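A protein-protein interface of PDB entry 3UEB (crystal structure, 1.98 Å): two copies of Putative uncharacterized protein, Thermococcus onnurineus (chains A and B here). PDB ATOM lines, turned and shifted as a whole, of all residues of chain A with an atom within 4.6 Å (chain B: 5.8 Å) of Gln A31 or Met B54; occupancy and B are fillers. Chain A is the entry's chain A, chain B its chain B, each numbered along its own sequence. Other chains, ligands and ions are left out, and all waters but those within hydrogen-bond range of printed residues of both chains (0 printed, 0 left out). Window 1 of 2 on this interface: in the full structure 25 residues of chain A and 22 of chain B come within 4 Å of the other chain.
N of Met A54 lies within hydrogen-bond range of O of Val B52 (2.9 Å). The backbone NH (N) of Met B54 lies within hydrogen-bond range of the backbone carbonyl oxygen (O) of Val A52. The side-chain amide oxygen (OE1) of Gln A31 is in hydrogen-bond range of the side-chain amide nitrogen (NE2) of Gln B31, at 2.5 Å. The backbone NH (N) of Ile B56 is in hydrogen-bond range of the backbone carbonyl oxygen (O) of Ile A50, at 3.0 Å. The side-chain carboxylate (OE2) of Glu A51 is in salt-bridge range of the guanidinium group (NE) of Arg B55, at 3.7 Å.
The guanidinium group (NH1) of Arg B55 is in salt-bridge range of the side-chain carboxylate (OE1) of Glu B65 (2.6 Å). The backbone carbonyl oxygen (O) of Glu B67 sits at hydrogen-bond distance from the backbone NH (N) of Thr B53 (2.9 Å). The backbone NH (N) of Glu A28 lies close to the side-chain sulfur (SD) of Met A54 (3.8 Å). NH2 of Arg B55 lies within salt-bridge range of OE1 of Glu B67 (2.7 Å). NE2 of Gln A31 is in hydrogen-bond range of O of Val A52.
Among the printed residues, pairs that only touch across the chains: Gln A31 with Met B54 (3.8 Å), Glu A32 with Glu B28 (3.4 Å), Ile A35 with Met B54 (3.4 Å), Ile A50 with Met B54 (3.7 Å), Ile A50 with Arg B55 (3.4 Å), Glu A51 with Met B54 (3.3 Å), Val A52 with Val B52 (3.8 Å), Val A52 with Thr B53 (3.5 Å) and Met A54 with Gln B31 (3.7 Å).
Of chain B, only Gln B31 (2.5 Å) and Met B54 (3.8 Å) come within 4 Å of Gln A31. Met B54 touches just these residues of chain A: Gln A31, Ile A35, Ile A50, Glu A51 and Val A52. Printed residues of chain A within 4 Å of Val B52: Val A52 (3.8 Å) and Met A54 (2.9 Å). Of the printed residues of chain B, Val A52 touches Val B52, Thr B53 and Met B54. The nearest printed residue of chain A that does not touch Met B54 is Glu A32 (5.3 Å).
Hydrophobic or aromatic side chains of chain A within 4 Å of the printed part of chain B: Ile A35, Ile A50 and Met A54. Hydrophobic or aromatic side chains of chain B that line the printed part of chain A: Met B54 and Ile B56. Among the printed residues, 14 pairs touch across the chains. Among the printed residues, Asp or Glu carboxylates within 4 Å of a Lys or Arg side-chain nitrogen of the other chain: Glu A51 with Arg B55.
Gln A31 touches its own counterpart, Gln B31. Gln A31 touches Met B54, and with the chains exchanged Met A54 touches Gln B31. Val B52 touches its own counterpart, Val A52. Val A52 touches Met B54, and with the chains exchanged Met A54 touches Val B52. Of the 14 pairs that touch across the chains among the printed residues, 6 have their exchanged pair printed and touching as well.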
ATOM      1  N   GLY A  27       2.088 -14.681 -22.236  1.00  0.00           N
ATOM      2  CA  GLY A  27       1.975 -15.510 -21.054  1.00  0.00           C
ATOM      3  C   GLY A  27       3.372 -15.802 -20.536  1.00  0.00           C
ATOM      4  O   GLY A  27       3.624 -15.738 -19.332  1.00  0.00           O
ATOM      5  N   GLU A  28       4.284 -16.116 -21.453  1.00  0.00           N
ATOM      6  CA  GLU A  28       5.664 -16.406 -21.088  1.00  0.00           C
ATOM      7  C   GLU A  28       6.354 -15.154 -20.544  1.00  0.00           C
ATOM      8  O   GLU A  28       7.081 -15.216 -19.553  1.00  0.00           O
ATOM      9  CB  GLU A  28       6.434 -16.934 -22.302  1.00  0.00           C
ATOM     10  CG  GLU A  28       6.017 -18.321 -22.757  1.00  0.00           C
ATOM     11  CD  GLU A  28       6.726 -18.760 -24.033  1.00  0.00           C
ATOM     12  OE1 GLU A  28       6.520 -19.912 -24.462  1.00  0.00           O
ATOM     13  OE2 GLU A  28       7.484 -17.954 -24.608  1.00  0.00           O
ATOM     14  N   LEU A  29       6.127 -14.017 -21.194  1.00  0.00           N
ATOM     15  CA  LEU A  29       6.739 -12.765 -20.753  1.00  0.00           C
ATOM     16  C   LEU A  29       6.300 -12.438 -19.323  1.00  0.00           C
ATOM     17  O   LEU A  29       7.115 -12.057 -18.472  1.00  0.00           O
ATOM     18  CB  LEU A  29       6.341 -11.624 -21.694  1.00  0.00           C
ATOM     19  CG  LEU A  29       6.911 -10.233 -21.388  1.00  0.00           C
ATOM     20  CD1 LEU A  29       8.442 -10.294 -21.330  1.00  0.00           C
ATOM     21  CD2 LEU A  29       6.460  -9.240 -22.461  1.00  0.00           C
ATOM     22  N   ALA A  30       5.011 -12.610 -19.065  1.00  0.00           N
ATOM     23  CA  ALA A  30       4.429 -12.335 -17.758  1.00  0.00           C
ATOM     24  C   ALA A  30       5.022 -13.224 -16.675  1.00  0.00           C
ATOM     25  O   ALA A  30       5.577 -12.734 -15.692  1.00  0.00           O
ATOM     26  CB  ALA A  30       2.918 -12.535 -17.818  1.00  0.00           C
ATOM     27  N   GLN A  31       4.901 -14.536 -16.872  1.00  0.00           N
ATOM     28  CA  GLN A  31       5.400 -15.520 -15.920  1.00  0.00           C
ATOM     29  C   GLN A  31       6.877 -15.352 -15.596  1.00  0.00           C
ATOM     30  O   GLN A  31       7.277 -15.379 -14.431  1.00  0.00           O
ATOM     31  CB  GLN A  31       5.177 -16.932 -16.456  1.00  0.00           C
ATOM     32  CG  GLN A  31       5.731 -18.016 -15.536  1.00  0.00           C
ATOM     33  CD  GLN A  31       6.204 -19.234 -16.296  1.00  0.00           C
ATOM     34  OE1 GLN A  31       6.830 -19.111 -17.345  1.00  0.00           O
ATOM     35  NE2 GLN A  31       5.928 -20.418 -15.757  1.00  0.00           N
ATOM     36  N   GLU A  32       7.685 -15.181 -16.635  1.00  0.00           N
ATOM     37  CA  GLU A  32       9.121 -15.035 -16.466  1.00  0.00           C
ATOM     38  C   GLU A  32       9.517 -13.688 -15.869  1.00  0.00           C
ATOM     39  O   GLU A  32      10.542 -13.577 -15.202  1.00  0.00           O
ATOM     40  CB  GLU A  32       9.811 -15.304 -17.809  1.00  0.00           C
ATOM     41  CG  GLU A  32       9.420 -16.688 -18.345  1.00  0.00           C
ATOM     42  CD  GLU A  32      10.002 -17.016 -19.706  1.00  0.00           C
ATOM     43  OE1 GLU A  32      10.540 -16.098 -20.364  1.00  0.00           O
ATOM     44  OE2 GLU A  32       9.904 -18.202 -20.113  1.00  0.00           O
ATOM     45  N   THR A  33       8.709 -12.660 -16.101  1.00  0.00           N
ATOM     46  CA  THR A  33       9.003 -11.362 -15.506  1.00  0.00           C
ATOM     47  C   THR A  33       8.857 -11.561 -13.993  1.00  0.00           C
ATOM     48  O   THR A  33       9.648 -11.053 -13.207  1.00  0.00           O
ATOM     49  CB  THR A  33       7.999 -10.275 -15.975  1.00  0.00           C
ATOM     50  OG1 THR A  33       8.199 -10.011 -17.374  1.00  0.00           O
ATOM     51  CG2 THR A  33       8.188  -8.983 -15.179  1.00  0.00           C
ATOM     52  N   ILE A  34       7.841 -12.318 -13.598  1.00  0.00           N
ATOM     53  CA  ILE A  34       7.588 -12.581 -12.189  1.00  0.00           C
ATOM     54  C   ILE A  34       8.692 -13.438 -11.564  1.00  0.00           C
ATOM     55  O   ILE A  34       9.116 -13.178 -10.436  1.00  0.00           O
ATOM     56  CB  ILE A  34       6.217 -13.264 -12.004  1.00  0.00           C
ATOM     57  CG1 ILE A  34       5.108 -12.290 -12.422  1.00  0.00           C
ATOM     58  CG2 ILE A  34       6.034 -13.701 -10.552  1.00  0.00           C
ATOM     59  CD1 ILE A  34       3.704 -12.870 -12.393  1.00  0.00           C
ATOM     60  N   ILE A  35       9.162 -14.447 -12.296  1.00  0.00           N
ATOM     61  CA  ILE A  35      10.228 -15.321 -11.800  1.00  0.00           C
ATOM     62  C   ILE A  35      11.511 -14.505 -11.639  1.00  0.00           C
ATOM     63  O   ILE A  35      12.195 -14.582 -10.614  1.00  0.00           O
ATOM     64  CB  ILE A  35      10.512 -16.492 -12.778  1.00  0.00           C
ATOM     65  CG1 ILE A  35       9.271 -17.366 -12.918  1.00  0.00           C
ATOM     66  CG2 ILE A  35      11.686 -17.334 -12.278  1.00  0.00           C
ATOM     67  CD1 ILE A  35       9.368 -18.373 -14.058  1.00  0.00           C
ATOM     68  N   ILE A  50       9.128 -21.669  -5.123  1.00  0.00           N
ATOM     69  CA  ILE A  50       8.439 -20.732  -5.979  1.00  0.00           C
ATOM     70  C   ILE A  50       7.743 -21.497  -7.101  1.00  0.00           C
ATOM     71  O   ILE A  50       8.305 -22.436  -7.679  1.00  0.00           O
ATOM     72  CB  ILE A  50       9.404 -19.671  -6.568  1.00  0.00           C
ATOM     73  CG1 ILE A  50       8.623 -18.728  -7.484  1.00  0.00           C
ATOM     74  CG2 ILE A  50      10.560 -20.335  -7.308  1.00  0.00           C
ATOM     75  CD1 ILE A  50       9.492 -17.676  -8.175  1.00  0.00           C
ATOM     76  N   GLU A  51       6.505 -21.107  -7.385  1.00  0.00           N
ATOM     77  CA  GLU A  51       5.733 -21.746  -8.441  1.00  0.00           C
ATOM     78  C   GLU A  51       4.943 -20.696  -9.198  1.00  0.00           C
ATOM     79  O   GLU A  51       4.132 -19.972  -8.617  1.00  0.00           O
ATOM     80  CB  GLU A  51       4.774 -22.781  -7.852  1.00  0.00           C
ATOM     81  CG  GLU A  51       5.449 -23.740  -6.905  1.00  0.00           C
ATOM     82  CD  GLU A  51       4.491 -24.745  -6.319  1.00  0.00           C
ATOM     83  OE1 GLU A  51       4.899 -25.457  -5.377  1.00  0.00           O
ATOM     84  OE2 GLU A  51       3.336 -24.824  -6.802  1.00  0.00           O
ATOM     85  N   VAL A  52       5.191 -20.614 -10.497  1.00  0.00           N
ATOM     86  CA  VAL A  52       4.503 -19.662 -11.335  1.00  0.00           C
ATOM     87  C   VAL A  52       3.861 -20.407 -12.500  1.00  0.00           C
ATOM     88  O   VAL A  52       4.532 -21.074 -13.295  1.00  0.00           O
ATOM     89  CB  VAL A  52       5.467 -18.589 -11.842  1.00  0.00           C
ATOM     90  CG1 VAL A  52       4.683 -17.486 -12.534  1.00  0.00           C
ATOM     91  CG2 VAL A  52       6.264 -18.016 -10.661  1.00  0.00           C
ATOM     92  N   MET A  54       1.202 -20.437 -15.891  1.00  0.00           N
ATOM     93  CA  MET A  54       0.583 -19.650 -16.949  1.00  0.00           C
ATOM     94  C   MET A  54      -0.459 -20.583 -17.554  1.00  0.00           C
ATOM     95  O   MET A  54      -0.180 -21.760 -17.818  1.00  0.00           O
ATOM     96  CB  MET A  54       1.588 -19.195 -18.019  1.00  0.00           C
ATOM     97  CG  MET A  54       1.938 -20.219 -19.096  1.00  0.00           C
ATOM     98  SD  MET A  54       2.892 -19.472 -20.429  1.00  0.00           S
ATOM     99  CE  MET A  54       4.471 -19.416 -19.640  1.00  0.00           C
ATOM    100  N   ILE A  66      -2.492 -16.158 -14.637  1.00  0.00           N
ATOM    101  CA  ILE A  66      -1.174 -16.350 -14.055  1.00  0.00           C
ATOM    102  C   ILE A  66      -1.345 -16.602 -12.575  1.00  0.00           C
ATOM    103  O   ILE A  66      -2.032 -15.852 -11.885  1.00  0.00           O
ATOM    104  CB  ILE A  66      -0.291 -15.108 -14.231  1.00  0.00           C
ATOM    105  CG1 ILE A  66       0.006 -14.877 -15.713  1.00  0.00           C
ATOM    106  CG2 ILE A  66       0.985 -15.267 -13.427  1.00  0.00           C
ATOM    107  CD1 ILE A  66       0.798 -15.991 -16.370  1.00  0.00           C
ATOM    108  N   ILE B  24      17.622 -19.836 -13.834  1.00  0.00           N
ATOM    109  CA  ILE B  24      16.490 -19.307 -14.569  1.00  0.00           C
ATOM    110  C   ILE B  24      16.522 -19.775 -16.025  1.00  0.00           C
ATOM    111  O   ILE B  24      15.484 -20.103 -16.591  1.00  0.00           O
ATOM    112  CB  ILE B  24      16.470 -17.764 -14.501  1.00  0.00           C
ATOM    113  CG1 ILE B  24      16.273 -17.324 -13.045  1.00  0.00           C
ATOM    114  CG2 ILE B  24      15.368 -17.215 -15.400  1.00  0.00           C
ATOM    115  CD1 ILE B  24      16.332 -15.826 -12.831  1.00  0.00           C
ATOM    116  N   GLY B  27      15.309 -23.429 -16.147  1.00  0.00           N
ATOM    117  CA  GLY B  27      13.879 -23.521 -15.912  1.00  0.00           C
ATOM    118  C   GLY B  27      13.101 -23.120 -17.154  1.00  0.00           C
ATOM    119  O   GLY B  27      12.209 -23.841 -17.595  1.00  0.00           O
ATOM    120  N   GLU B  28      13.448 -21.972 -17.731  1.00  0.00           N
ATOM    121  CA  GLU B  28      12.759 -21.489 -18.922  1.00  0.00           C
ATOM    122  C   GLU B  28      12.983 -22.396 -20.123  1.00  0.00           C
ATOM    123  O   GLU B  28      12.088 -22.569 -20.947  1.00  0.00           O
ATOM    124  CB  GLU B  28      13.200 -20.054 -19.246  1.00  0.00           C
ATOM    125  CG  GLU B  28      13.084 -19.113 -18.045  1.00  0.00           C
ATOM    126  CD  GLU B  28      13.378 -17.663 -18.373  1.00  0.00           C
ATOM    127  OE1 GLU B  28      14.105 -17.403 -19.358  1.00  0.00           O
ATOM    128  OE2 GLU B  28      12.895 -16.781 -17.628  1.00  0.00           O
ATOM    129  N   GLN B  31      10.656 -25.472 -19.834  1.00  0.00           N
ATOM    130  CA  GLN B  31       9.278 -25.081 -20.083  1.00  0.00           C
ATOM    131  C   GLN B  31       8.995 -24.704 -21.538  1.00  0.00           C
ATOM    132  O   GLN B  31       7.983 -25.114 -22.113  1.00  0.00           O
ATOM    133  CB  GLN B  31       8.933 -23.923 -19.162  1.00  0.00           C
ATOM    134  CG  GLN B  31       7.515 -23.470 -19.227  1.00  0.00           C
ATOM    135  CD  GLN B  31       7.260 -22.365 -18.236  1.00  0.00           C
ATOM    136  OE1 GLN B  31       6.816 -22.608 -17.115  1.00  0.00           O
ATOM    137  NE2 GLN B  31       7.567 -21.138 -18.637  1.00  0.00           N
ATOM    138  N   VAL B  52       0.956 -24.481 -17.821  1.00  0.00           N
ATOM    139  CA  VAL B  52       2.332 -24.825 -17.509  1.00  0.00           C
ATOM    140  C   VAL B  52       2.801 -24.127 -16.242  1.00  0.00           C
ATOM    141  O   VAL B  52       2.691 -22.915 -16.120  1.00  0.00           O
ATOM    142  CB  VAL B  52       3.265 -24.433 -18.677  1.00  0.00           C
ATOM    143  CG1 VAL B  52       4.659 -24.959 -18.425  1.00  0.00           C
ATOM    144  CG2 VAL B  52       2.718 -24.988 -19.982  1.00  0.00           C
ATOM    145  N   THR B  53       3.336 -24.904 -15.308  1.00  0.00           N
ATOM    146  CA  THR B  53       3.830 -24.371 -14.045  1.00  0.00           C
ATOM    147  C   THR B  53       5.326 -24.655 -13.867  1.00  0.00           C
ATOM    148  O   THR B  53       5.761 -25.806 -13.984  1.00  0.00           O
ATOM    149  CB  THR B  53       3.073 -25.005 -12.842  1.00  0.00           C
ATOM    150  OG1 THR B  53       1.685 -24.663 -12.907  1.00  0.00           O
ATOM    151  CG2 THR B  53       3.653 -24.509 -11.510  1.00  0.00           C
ATOM    152  N   MET B  54       6.118 -23.611 -13.630  1.00  0.00           N
ATOM    153  CA  MET B  54       7.541 -23.808 -13.378  1.00  0.00           C
ATOM    154  C   MET B  54       7.626 -23.812 -11.862  1.00  0.00           C
ATOM    155  O   MET B  54       7.128 -22.899 -11.193  1.00  0.00           O
ATOM    156  CB  MET B  54       8.416 -22.676 -13.923  1.00  0.00           C
ATOM    157  CG  MET B  54       9.930 -22.951 -13.728  1.00  0.00           C
ATOM    158  SD  MET B  54      11.038 -21.551 -14.031  1.00  0.00           S
ATOM    159  CE  MET B  54      10.572 -21.113 -15.670  1.00  0.00           C
ATOM    160  N   ARG B  55       8.265 -24.840 -11.326  1.00  0.00           N
ATOM    161  CA  ARG B  55       8.377 -25.007  -9.893  1.00  0.00           C
ATOM    162  C   ARG B  55       9.838 -25.250  -9.521  1.00  0.00           C
ATOM    163  O   ARG B  55      10.501 -26.133 -10.071  1.00  0.00           O
ATOM    164  CB  ARG B  55       7.489 -26.193  -9.489  1.00  0.00           C
ATOM    165  CG  ARG B  55       7.373 -26.514  -8.017  1.00  0.00           C
ATOM    166  CD  ARG B  55       6.489 -27.764  -7.827  1.00  0.00           C
ATOM    167  NE  ARG B  55       5.154 -27.594  -8.412  1.00  0.00           N
ATOM    168  CZ  ARG B  55       4.549 -28.479  -9.208  1.00  0.00           C
ATOM    169  NH1 ARG B  55       5.151 -29.616  -9.533  1.00  0.00           N
ATOM    170  NH2 ARG B  55       3.334 -28.225  -9.686  1.00  0.00           N
ATOM    171  N   ILE B  56      10.345 -24.433  -8.604  1.00  0.00           N
ATOM    172  CA  ILE B  56      11.717 -24.556  -8.143  1.00  0.00           C
ATOM    173  C   ILE B  56      11.669 -24.693  -6.626  1.00  0.00           C
ATOM    174  O   ILE B  56      11.272 -23.765  -5.909  1.00  0.00           O
ATOM    175  CB  ILE B  56      12.547 -23.333  -8.569  1.00  0.00           C
ATOM    176  CG1 ILE B  56      12.590 -23.269 -10.102  1.00  0.00           C
ATOM    177  CG2 ILE B  56      13.961 -23.424  -8.006  1.00  0.00           C
ATOM    178  CD1 ILE B  56      13.455 -22.162 -10.663  1.00  0.00           C
ATOM    179  N   LEU B  64      13.830 -28.805  -9.903  1.00  0.00           N
ATOM    180  CA  LEU B  64      13.067 -28.071 -10.895  1.00  0.00           C
ATOM    181  C   LEU B  64      11.974 -28.986 -11.414  1.00  0.00           C
ATOM    182  O   LEU B  64      12.222 -30.146 -11.755  1.00  0.00           O
ATOM    183  CB  LEU B  64      13.941 -27.646 -12.074  1.00  0.00           C
ATOM    184  CG  LEU B  64      13.109 -27.181 -13.280  1.00  0.00           C
ATOM    185  CD1 LEU B  64      12.729 -25.724 -13.101  1.00  0.00           C
ATOM    186  CD2 LEU B  64      13.903 -27.362 -14.562  1.00  0.00           C
ATOM    187  N   GLU B  65      10.759 -28.467 -11.477  1.00  0.00           N
ATOM    188  CA  GLU B  65       9.650 -29.251 -11.984  1.00  0.00           C
ATOM    189  C   GLU B  65       8.845 -28.402 -12.942  1.00  0.00           C
ATOM    190  O   GLU B  65       8.571 -27.235 -12.666  1.00  0.00           O
ATOM    191  CB  GLU B  65       8.727 -29.720 -10.852  1.00  0.00           C
ATOM    192  CG  GLU B  65       9.354 -30.669  -9.845  1.00  0.00           C
ATOM    193  CD  GLU B  65       8.312 -31.435  -9.051  1.00  0.00           C
ATOM    194  OE1 GLU B  65       7.275 -30.830  -8.708  1.00  0.00           O
ATOM    195  OE2 GLU B  65       8.524 -32.637  -8.760  1.00  0.00           O
ATOM    196  N   ILE B  66       8.487 -28.982 -14.081  1.00  0.00           N
ATOM    197  CA  ILE B  66       7.655 -28.277 -15.032  1.00  0.00           C
ATOM    198  C   ILE B  66       6.438 -29.153 -15.177  1.00  0.00           C
ATOM    199  O   ILE B  66       6.526 -30.295 -15.639  1.00  0.00           O
ATOM    200  CB  ILE B  66       8.301 -28.113 -16.416  1.00  0.00           C
ATOM    201  CG1 ILE B  66       9.622 -27.341 -16.303  1.00  0.00           C
ATOM    202  CG2 ILE B  66       7.321 -27.383 -17.340  1.00  0.00           C
ATOM    203  CD1 ILE B  66       9.490 -25.935 -15.792  1.00  0.00           C
ATOM    204  N   GLU B  67       5.302 -28.631 -14.744  1.00  0.00           N
ATOM    205  CA  GLU B  67       4.060 -29.375 -14.837  1.00  0.00           C
ATOM    206  C   GLU B  67       3.254 -28.844 -16.013  1.00  0.00           C
ATOM    207  O   GLU B  67       3.001 -27.643 -16.119  1.00  0.00           O
ATOM    208  CB  GLU B  67       3.263 -29.250 -13.534  1.00  0.00           C
ATOM    209  CG  GLU B  67       1.840 -29.783 -13.630  1.00  0.00           C
ATOM    210  CD  GLU B  67       1.281 -30.236 -12.288  1.00  0.00           C
ATOM    211  OE1 GLU B  67       1.823 -29.820 -11.237  1.00  0.00           O
ATOM    212  OE2 GLU B  67       0.292 -31.003 -12.288  1.00  0.00           O
